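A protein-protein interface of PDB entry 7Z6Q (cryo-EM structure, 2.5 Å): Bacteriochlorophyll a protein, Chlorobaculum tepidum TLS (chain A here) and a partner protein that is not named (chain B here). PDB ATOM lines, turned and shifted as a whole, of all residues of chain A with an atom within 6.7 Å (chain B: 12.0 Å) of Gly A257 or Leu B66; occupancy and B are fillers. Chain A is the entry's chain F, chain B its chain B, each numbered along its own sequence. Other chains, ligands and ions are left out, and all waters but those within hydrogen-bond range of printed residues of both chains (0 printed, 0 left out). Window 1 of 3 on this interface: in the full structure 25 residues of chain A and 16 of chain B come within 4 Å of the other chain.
The backbone carbonyl oxygen (O) of Cys A49 sits at hydrogen-bond distance from the backbone NH (N) of Phe A258. The backbone NH of Gly A257 lies within hydrogen-bond range of the backbone carbonyl oxygen of Lys A268, at 2.8 Å. N of Arg A259 sits at hydrogen-bond distance from O of Glu A266.
Of the 14 printed residues of chain A, 6 touch a printed residue of chain B. Printed residues of chain B that touch a printed residue of chain A: Leu B63, Ala B64, Leu B66, Gly B67, Val B68 and Leu B70. Hydrophobic or aromatic side chains of chain B that line the printed part of chain A: Leu B63, Leu B66, Val B68 and Leu B70. Among the printed residues, 10 pairs touch across the chains. Among the printed residues, no Asp or Glu carboxylate lies within 4 Å of a Lys or Arg side-chain nitrogen of the other chain.
Among the printed residues, pairs that only touch across the chains: Arg A33 with Leu B70, Cys A49 with Leu B63, Gly A257 with Leu B66, Phe A258 with Leu B66, Arg A259 with Leu B63 and Arg A259 with Leu B66.
Printed residues of chain B within 4 Å of Gly A257: Leu B66. Of chain A, only Gly A257 (3.5 Å), Phe A258 (3.4 Å), Arg A259 (3.6 Å) and Glu A266 (2.4 Å) come within 4 Å of Leu B66. Of the printed residues of chain B, Cys A49 touches Leu B63 (3.9 Å). No residue of chain B comes within 4 Å of Ala A256. Of chain B, only Leu B66 (3.4 Å) comes within 4 Å of Phe A258. Arg A259 touches three residues of chain B. No residue of chain B comes within 4 Å of Val A267. No residue of chain B comes within 4 Å of Lys A268. Printed residues of chain B within 4 Å of Arg A33: Gly B67 (3.2 Å) and Leu B70 (3.2 Å). Of the printed residues of chain A, Gly B67 touches Arg A33. Of the printed residues of chain A, Ala B64 touches Arg A259 (2.5 Å). Of the printed residues of chain A, Leu B70 touches Arg A33 (3.2 Å). The nearest residue of chain A that does not touch Leu B66 is Lys A268 (4.1 Å).
The guanidinium group (NH1) of Arg A259 lies within hydrogen-bond range of the backbone carbonyl oxygen (O) of Ala B64, 2.5 Å away. The backbone carbonyl oxygen (O) of Leu B66 sits close to the side-chain carboxylate (OE2) of Glu A266, 2.4 Å away. O of Gly B67 lies within hydrogen-bond range of NH1 of Arg A33 (3.2 Å). The side-chain carboxylate of Glu A266 lies close to the backbone carbonyl oxygen of Val B68 (3.3 Å).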
ATOM      1  N   ARG A  33      19.040  20.480  16.318  1.00  0.00           N
ATOM      2  CA  ARG A  33      19.695  19.255  16.850  1.00  0.00           C
ATOM      3  C   ARG A  33      18.629  18.434  17.584  1.00  0.00           C
ATOM      4  O   ARG A  33      17.884  19.033  18.385  1.00  0.00           O
ATOM      5  CB  ARG A  33      20.848  19.628  17.787  1.00  0.00           C
ATOM      6  CG  ARG A  33      22.010  20.328  17.096  1.00  0.00           C
ATOM      7  CD  ARG A  33      23.158  20.614  18.045  1.00  0.00           C
ATOM      8  NE  ARG A  33      24.260  21.303  17.390  1.00  0.00           N
ATOM      9  CZ  ARG A  33      25.210  20.701  16.683  1.00  0.00           C
ATOM     10  NH1 ARG A  33      25.195  19.387  16.537  1.00  0.00           N
ATOM     11  NH2 ARG A  33      26.172  21.415  16.125  1.00  0.00           N
ATOM     12  N   CYS A  49      22.303   8.408   7.427  1.00  0.00           N
ATOM     13  CA  CYS A  49      22.148   9.205   6.177  1.00  0.00           C
ATOM     14  C   CYS A  49      22.609  10.655   6.348  1.00  0.00           C
ATOM     15  O   CYS A  49      22.175  11.307   7.310  1.00  0.00           O
ATOM     16  CB  CYS A  49      20.682   9.260   5.759  1.00  0.00           C
ATOM     17  SG  CYS A  49      20.392  10.244   4.267  1.00  0.00           S
ATOM     18  N   ASP A  50      23.417  11.139   5.398  1.00  0.00           N
ATOM     19  CA  ASP A  50      23.905  12.543   5.368  1.00  0.00           C
ATOM     20  C   ASP A  50      23.424  13.178   4.057  1.00  0.00           C
ATOM     21  O   ASP A  50      23.586  12.538   3.007  1.00  0.00           O
ATOM     22  CB  ASP A  50      25.423  12.623   5.556  1.00  0.00           C
ATOM     23  CG  ASP A  50      25.959  14.041   5.630  1.00  0.00           C
ATOM     24  OD1 ASP A  50      25.142  14.978   5.553  1.00  0.00           O
ATOM     25  OD2 ASP A  50      27.189  14.197   5.758  1.00  0.00           O
ATOM     26  N   VAL A  51      22.852  14.386   4.125  1.00  0.00           N
ATOM     27  CA  VAL A  51      22.319  15.081   2.912  1.00  0.00           C
ATOM     28  C   VAL A  51      22.936  16.483   2.818  1.00  0.00           C
ATOM     29  O   VAL A  51      23.042  17.151   3.866  1.00  0.00           O
ATOM     30  CB  VAL A  51      20.780  15.152   2.956  1.00  0.00           C
ATOM     31  CG1 VAL A  51      20.195  15.634   1.637  1.00  0.00           C
ATOM     32  CG2 VAL A  51      20.166  13.819   3.358  1.00  0.00           C
ATOM     33  N   GLU A 255      22.573  21.907   5.246  1.00  0.00           N
ATOM     34  CA  GLU A 255      23.320  20.645   5.486  1.00  0.00           C
ATOM     35  C   GLU A 255      22.668  19.908   6.655  1.00  0.00           C
ATOM     36  O   GLU A 255      22.448  20.546   7.698  1.00  0.00           O
ATOM     37  CB  GLU A 255      24.795  20.950   5.754  1.00  0.00           C
ATOM     38  CG  GLU A 255      25.637  21.006   4.493  1.00  0.00           C
ATOM     39  CD  GLU A 255      27.091  21.379   4.730  1.00  0.00           C
ATOM     40  OE1 GLU A 255      27.415  21.783   5.863  1.00  0.00           O
ATOM     41  OE2 GLU A 255      27.892  21.266   3.781  1.00  0.00           O
ATOM     42  N   ALA A 256      22.387  18.618   6.483  1.00  0.00           N
ATOM     43  CA  ALA A 256      21.748  17.827   7.557  1.00  0.00           C
ATOM     44  C   ALA A 256      22.235  16.379   7.488  1.00  0.00           C
ATOM     45  O   ALA A 256      22.879  16.024   6.494  1.00  0.00           O
ATOM     46  CB  ALA A 256      20.248  17.905   7.421  1.00  0.00           C
ATOM     47  N   GLY A 257      21.972  15.602   8.539  1.00  0.00           N
ATOM     48  CA  GLY A 257      22.340  14.174   8.585  1.00  0.00           C
ATOM     49  C   GLY A 257      21.679  13.479   9.761  1.00  0.00           C
ATOM     50  O   GLY A 257      21.261  14.190  10.683  1.00  0.00           O
ATOM     51  N   PHE A 258      21.600  12.146   9.747  1.00  0.00           N
ATOM     52  CA  PHE A 258      20.967  11.437  10.890  1.00  0.00           C
ATOM     53  C   PHE A 258      21.520  10.015  11.034  1.00  0.00           C
ATOM     54  O   PHE A 258      21.953   9.425  10.037  1.00  0.00           O
ATOM     55  CB  PHE A 258      19.440  11.433  10.759  1.00  0.00           C
ATOM     56  CG  PHE A 258      18.894  10.517   9.693  1.00  0.00           C
ATOM     57  CD1 PHE A 258      18.956   9.142   9.840  1.00  0.00           C
ATOM     58  CD2 PHE A 258      18.310  11.030   8.547  1.00  0.00           C
ATOM     59  CE1 PHE A 258      18.452   8.300   8.862  1.00  0.00           C
ATOM     60  CE2 PHE A 258      17.804  10.187   7.571  1.00  0.00           C
ATOM     61  CZ  PHE A 258      17.874   8.824   7.730  1.00  0.00           C
ATOM     62  N   ARG A 259      21.493   9.517  12.267  1.00  0.00           N
ATOM     63  CA  ARG A 259      21.949   8.147  12.579  1.00  0.00           C
ATOM     64  C   ARG A 259      20.744   7.415  13.158  1.00  0.00           C
ATOM     65  O   ARG A 259      20.015   8.020  13.948  1.00  0.00           O
ATOM     66  CB  ARG A 259      23.116   8.196  13.566  1.00  0.00           C
ATOM     67  CG  ARG A 259      24.239   9.122  13.131  1.00  0.00           C
ATOM     68  CD  ARG A 259      24.816   8.660  11.816  1.00  0.00           C
ATOM     69  NE  ARG A 259      25.911   9.480  11.328  1.00  0.00           N
ATOM     70  CZ  ARG A 259      25.812  10.315  10.303  1.00  0.00           C
ATOM     71  NH1 ARG A 259      26.864  11.013   9.912  1.00  0.00           N
ATOM     72  NH2 ARG A 259      24.659  10.454   9.677  1.00  0.00           N
ATOM     73  N   GLU A 266      19.517  10.027  15.887  1.00  0.00           N
ATOM     74  CA  GLU A 266      20.263  11.228  16.206  1.00  0.00           C
ATOM     75  C   GLU A 266      20.206  12.062  14.940  1.00  0.00           C
ATOM     76  O   GLU A 266      20.509  11.565  13.879  1.00  0.00           O
ATOM     77  CB  GLU A 266      21.693  10.878  16.593  1.00  0.00           C
ATOM     78  CG  GLU A 266      22.518  12.077  17.038  1.00  0.00           C
ATOM     79  CD  GLU A 266      23.866  11.696  17.631  1.00  0.00           C
ATOM     80  OE1 GLU A 266      24.001  11.742  18.870  1.00  0.00           O
ATOM     81  OE2 GLU A 266      24.787  11.334  16.868  1.00  0.00           O
ATOM     82  N   VAL A 267      19.788  13.335  15.044  1.00  0.00           N
ATOM     83  CA  VAL A 267      19.641  14.167  13.811  1.00  0.00           C
ATOM     84  C   VAL A 267      20.327  15.529  13.980  1.00  0.00           C
ATOM     85  O   VAL A 267      20.166  16.147  15.051  1.00  0.00           O
ATOM     86  CB  VAL A 267      18.154  14.337  13.432  1.00  0.00           C
ATOM     87  CG1 VAL A 267      17.966  15.268  12.244  1.00  0.00           C
ATOM     88  CG2 VAL A 267      17.472  13.001  13.173  1.00  0.00           C
ATOM     89  N   LYS A 268      21.058  15.965  12.946  1.00  0.00           N
ATOM     90  CA  LYS A 268      21.716  17.271  12.936  1.00  0.00           C
ATOM     91  C   LYS A 268      21.344  18.033  11.657  1.00  0.00           C
ATOM     92  O   LYS A 268      21.469  17.492  10.559  1.00  0.00           O
ATOM     93  CB  LYS A 268      23.234  17.110  13.030  1.00  0.00           C
ATOM     94  CG  LYS A 268      23.997  18.423  13.098  1.00  0.00           C
ATOM     95  CD  LYS A 268      25.492  18.186  13.239  1.00  0.00           C
ATOM     96  CE  LYS A 268      26.258  19.499  13.282  1.00  0.00           C
ATOM     97  NZ  LYS A 268      27.725  19.282  13.421  1.00  0.00           N
ATOM     98  N   VAL A 269      20.890  19.279  11.792  1.00  0.00           N
ATOM     99  CA  VAL A 269      20.506  20.062  10.622  1.00  0.00           C
ATOM    100  C   VAL A 269      20.991  21.509  10.724  1.00  0.00           C
ATOM    101  O   VAL A 269      20.834  22.120  11.762  1.00  0.00           O
ATOM    102  CB  VAL A 269      18.959  20.061  10.469  1.00  0.00           C
ATOM    103  CG1 VAL A 269      18.491  20.834   9.249  1.00  0.00           C
ATOM    104  CG2 VAL A 269      18.400  18.651  10.447  1.00  0.00           C
ATOM    105  N   ASP A 270      21.573  22.069   9.660  1.00  0.00           N
ATOM    106  CA  ASP A 270      22.032  23.468   9.689  1.00  0.00           C
ATOM    107  C   ASP A 270      22.146  24.106   8.293  1.00  0.00           C
ATOM    108  O   ASP A 270      22.424  23.406   7.319  1.00  0.00           O
ATOM    109  CB  ASP A 270      23.373  23.576  10.420  1.00  0.00           C
ATOM    110  CG  ASP A 270      24.492  22.856   9.694  1.00  0.00           C
ATOM    111  OD1 ASP A 270      24.273  22.419   8.545  1.00  0.00           O
ATOM    112  OD2 ASP A 270      25.591  22.726  10.273  1.00  0.00           O
ATOM    113  N   ARG B  62      29.240   2.167   9.497  1.00  0.00           N
ATOM    114  CA  ARG B  62      28.413   3.388   9.684  1.00  0.00           C
ATOM    115  C   ARG B  62      29.171   4.601   9.135  1.00  0.00           C
ATOM    116  O   ARG B  62      30.353   4.453   8.778  1.00  0.00           O
ATOM    117  CB  ARG B  62      28.057   3.575  11.162  1.00  0.00           C
ATOM    118  CG  ARG B  62      27.040   2.581  11.701  1.00  0.00           C
ATOM    119  CD  ARG B  62      25.885   3.302  12.365  1.00  0.00           C
ATOM    120  NE  ARG B  62      25.157   2.490  13.325  1.00  0.00           N
ATOM    121  CZ  ARG B  62      24.114   2.924  14.022  1.00  0.00           C
ATOM    122  NH1 ARG B  62      23.505   2.123  14.880  1.00  0.00           N
ATOM    123  NH2 ARG B  62      23.685   4.163  13.857  1.00  0.00           N
ATOM    124  N   LEU B  63      28.487   5.744   9.068  1.00  0.00           N
ATOM    125  CA  LEU B  63      29.043   7.032   8.576  1.00  0.00           C
ATOM    126  C   LEU B  63      29.700   7.770   9.749  1.00  0.00           C
ATOM    127  O   LEU B  63      29.529   7.327  10.902  1.00  0.00           O
ATOM    128  CB  LEU B  63      27.910   7.864   7.965  1.00  0.00           C
ATOM    129  CG  LEU B  63      27.266   7.273   6.712  1.00  0.00           C
ATOM    130  CD1 LEU B  63      26.065   8.100   6.278  1.00  0.00           C
ATOM    131  CD2 LEU B  63      28.278   7.169   5.580  1.00  0.00           C
ATOM    132  N   ALA B  64      30.401   8.872   9.466  1.00  0.00           N
ATOM    133  CA  ALA B  64      31.088   9.618  10.545  1.00  0.00           C
ATOM    134  C   ALA B  64      30.039  10.047  11.578  1.00  0.00           C
ATOM    135  O   ALA B  64      28.975  10.559  11.180  1.00  0.00           O
ATOM    136  CB  ALA B  64      31.818  10.806   9.969  1.00  0.00           C
ATOM    137  N   SER B  65      30.359   9.869  12.861  1.00  0.00           N
ATOM    138  CA  SER B  65      29.424  10.155  13.981  1.00  0.00           C
ATOM    139  C   SER B  65      28.934  11.608  13.991  1.00  0.00           C
ATOM    140  O   SER B  65      29.703  12.514  13.618  1.00  0.00           O
ATOM    141  CB  SER B  65      30.047   9.791  15.302  1.00  0.00           C
ATOM    142  OG  SER B  65      31.258  10.506  15.497  1.00  0.00           O
ATOM    143  N   LEU B  66      27.678  11.781  14.410  1.00  0.00           N
ATOM    144  CA  LEU B  66      27.014  13.067  14.591  1.00  0.00           C
ATOM    145  C   LEU B  66      27.190  13.468  16.050  1.00  0.00           C
ATOM    146  O   LEU B  66      26.720  12.761  16.950  1.00  0.00           O
ATOM    147  CB  LEU B  66      25.523  13.012  14.248  1.00  0.00           C
ATOM    148  CG  LEU B  66      24.942  12.742  12.854  1.00  0.00           C
ATOM    149  CD1 LEU B  66      23.430  12.623  12.960  1.00  0.00           C
ATOM    150  CD2 LEU B  66      25.338  13.729  11.770  1.00  0.00           C
ATOM    151  N   GLY B  67      27.843  14.601  16.286  1.00  0.00           N
ATOM    152  CA  GLY B  67      28.092  15.016  17.650  1.00  0.00           C
ATOM    153  C   GLY B  67      26.900  15.761  18.204  1.00  0.00           C
ATOM    154  O   GLY B  67      26.741  16.967  17.991  1.00  0.00           O
ATOM    155  N   VAL B  68      26.055  15.035  18.930  1.00  0.00           N
ATOM    156  CA  VAL B  68      24.787  15.544  19.434  1.00  0.00           C
ATOM    157  C   VAL B  68      24.720  15.162  20.906  1.00  0.00           C
ATOM    158  O   VAL B  68      24.415  14.013  21.243  1.00  0.00           O
ATOM    159  CB  VAL B  68      23.585  14.990  18.661  1.00  0.00           C
ATOM    160  CG1 VAL B  68      22.286  15.488  19.269  1.00  0.00           C
ATOM    161  CG2 VAL B  68      23.670  15.380  17.195  1.00  0.00           C
ATOM    162  N   THR B  69      25.010  16.117  21.783  1.00  0.00           N
ATOM    163  CA  THR B  69      24.967  15.917  23.227  1.00  0.00           C
ATOM    164  C   THR B  69      23.844  16.800  23.763  1.00  0.00           C
ATOM    165  O   THR B  69      24.072  17.948  24.150  1.00  0.00           O
ATOM    166  CB  THR B  69      26.309  16.250  23.873  1.00  0.00           C
ATOM    167  OG1 THR B  69      26.661  17.608  23.576  1.00  0.00           O
ATOM    168  CG2 THR B  69      27.394  15.327  23.342  1.00  0.00           C
ATOM    169  N   LEU B  70      22.622  16.256  23.770  1.00  0.00           N
ATOM    170  CA  LEU B  70      21.426  17.037  24.191  1.00  0.00           C
ATOM    171  C   LEU B  70      20.890  16.576  25.552  1.00  0.00           C
ATOM    172  O   LEU B  70      20.489  17.453  26.343  1.00  0.00           O
ATOM    173  CB  LEU B  70      20.349  16.915  23.109  1.00  0.00           C
ATOM    174  CG  LEU B  70      20.591  17.737  21.844  1.00  0.00           C
ATOM    175  CD1 LEU B  70      19.375  17.699  20.932  1.00  0.00           C
ATOM    176  CD2 LEU B  70      20.951  19.173  22.192  1.00  0.00           C
ATOM    177  N   GLY B  71      20.878  15.265  25.823  1.00  0.00           N
ATOM    178  CA  GLY B  71      20.340  14.787  27.079  1.00  0.00           C
ATOM    179  C   GLY B  71      21.369  14.715  28.183  1.00  0.00           C
ATOM    180  O   GLY B  71      22.202  15.617  28.326  1.00  0.00           O
ATOM    181  N   SER B  73      24.415  14.014  29.541  1.00  0.00           N
ATOM    182  CA  SER B  73      25.737  13.824  28.895  1.00  0.00           C
ATOM    183  C   SER B  73      26.736  14.667  29.695  1.00  0.00           C
ATOM    184  O   SER B  73      26.322  15.679  30.300  1.00  0.00           O
ATOM    185  CB  SER B  73      25.820  14.124  27.422  1.00  0.00           C
ATOM    186  OG  SER B  73      25.255  15.390  27.133  1.00  0.00           O
ATOM    187  N   VAL B  75      28.978  16.310  28.608  1.00  0.00           N
ATOM    188  CA  VAL B  75      29.427  17.431  27.731  1.00  0.00           C
ATOM    189  C   VAL B  75      28.716  18.721  28.146  1.00  0.00           C
ATOM    190  O   VAL B  75      27.542  18.654  28.557  1.00  0.00           O
ATOM    191  CB  VAL B  75      29.191  17.117  26.244  1.00  0.00           C
ATOM    192  CG1 VAL B  75      29.889  18.126  25.346  1.00  0.00           C
ATOM    193  CG2 VAL B  75      29.624  15.702  25.901  1.00  0.00           C
ATOM    194  N   GLN B  77      26.656  22.156  27.703  1.00  0.00           N
ATOM    195  CA  GLN B  77      25.587  22.675  26.795  1.00  0.00           C
ATOM    196  C   GLN B  77      25.880  24.136  26.416  1.00  0.00           C
ATOM    197  O   GLN B  77      26.830  24.711  26.981  1.00  0.00           O
ATOM    198  CB  GLN B  77      24.195  22.511  27.411  1.00  0.00           C
ATOM    199  CG  GLN B  77      23.760  21.061  27.582  1.00  0.00           C
ATOM    200  CD  GLN B  77      23.702  20.289  26.287  1.00  0.00           C
ATOM    201  OE1 GLN B  77      23.272  20.796  25.255  1.00  0.00           O
ATOM    202  NE2 GLN B  77      24.145  19.045  26.330  1.00  0.00           N
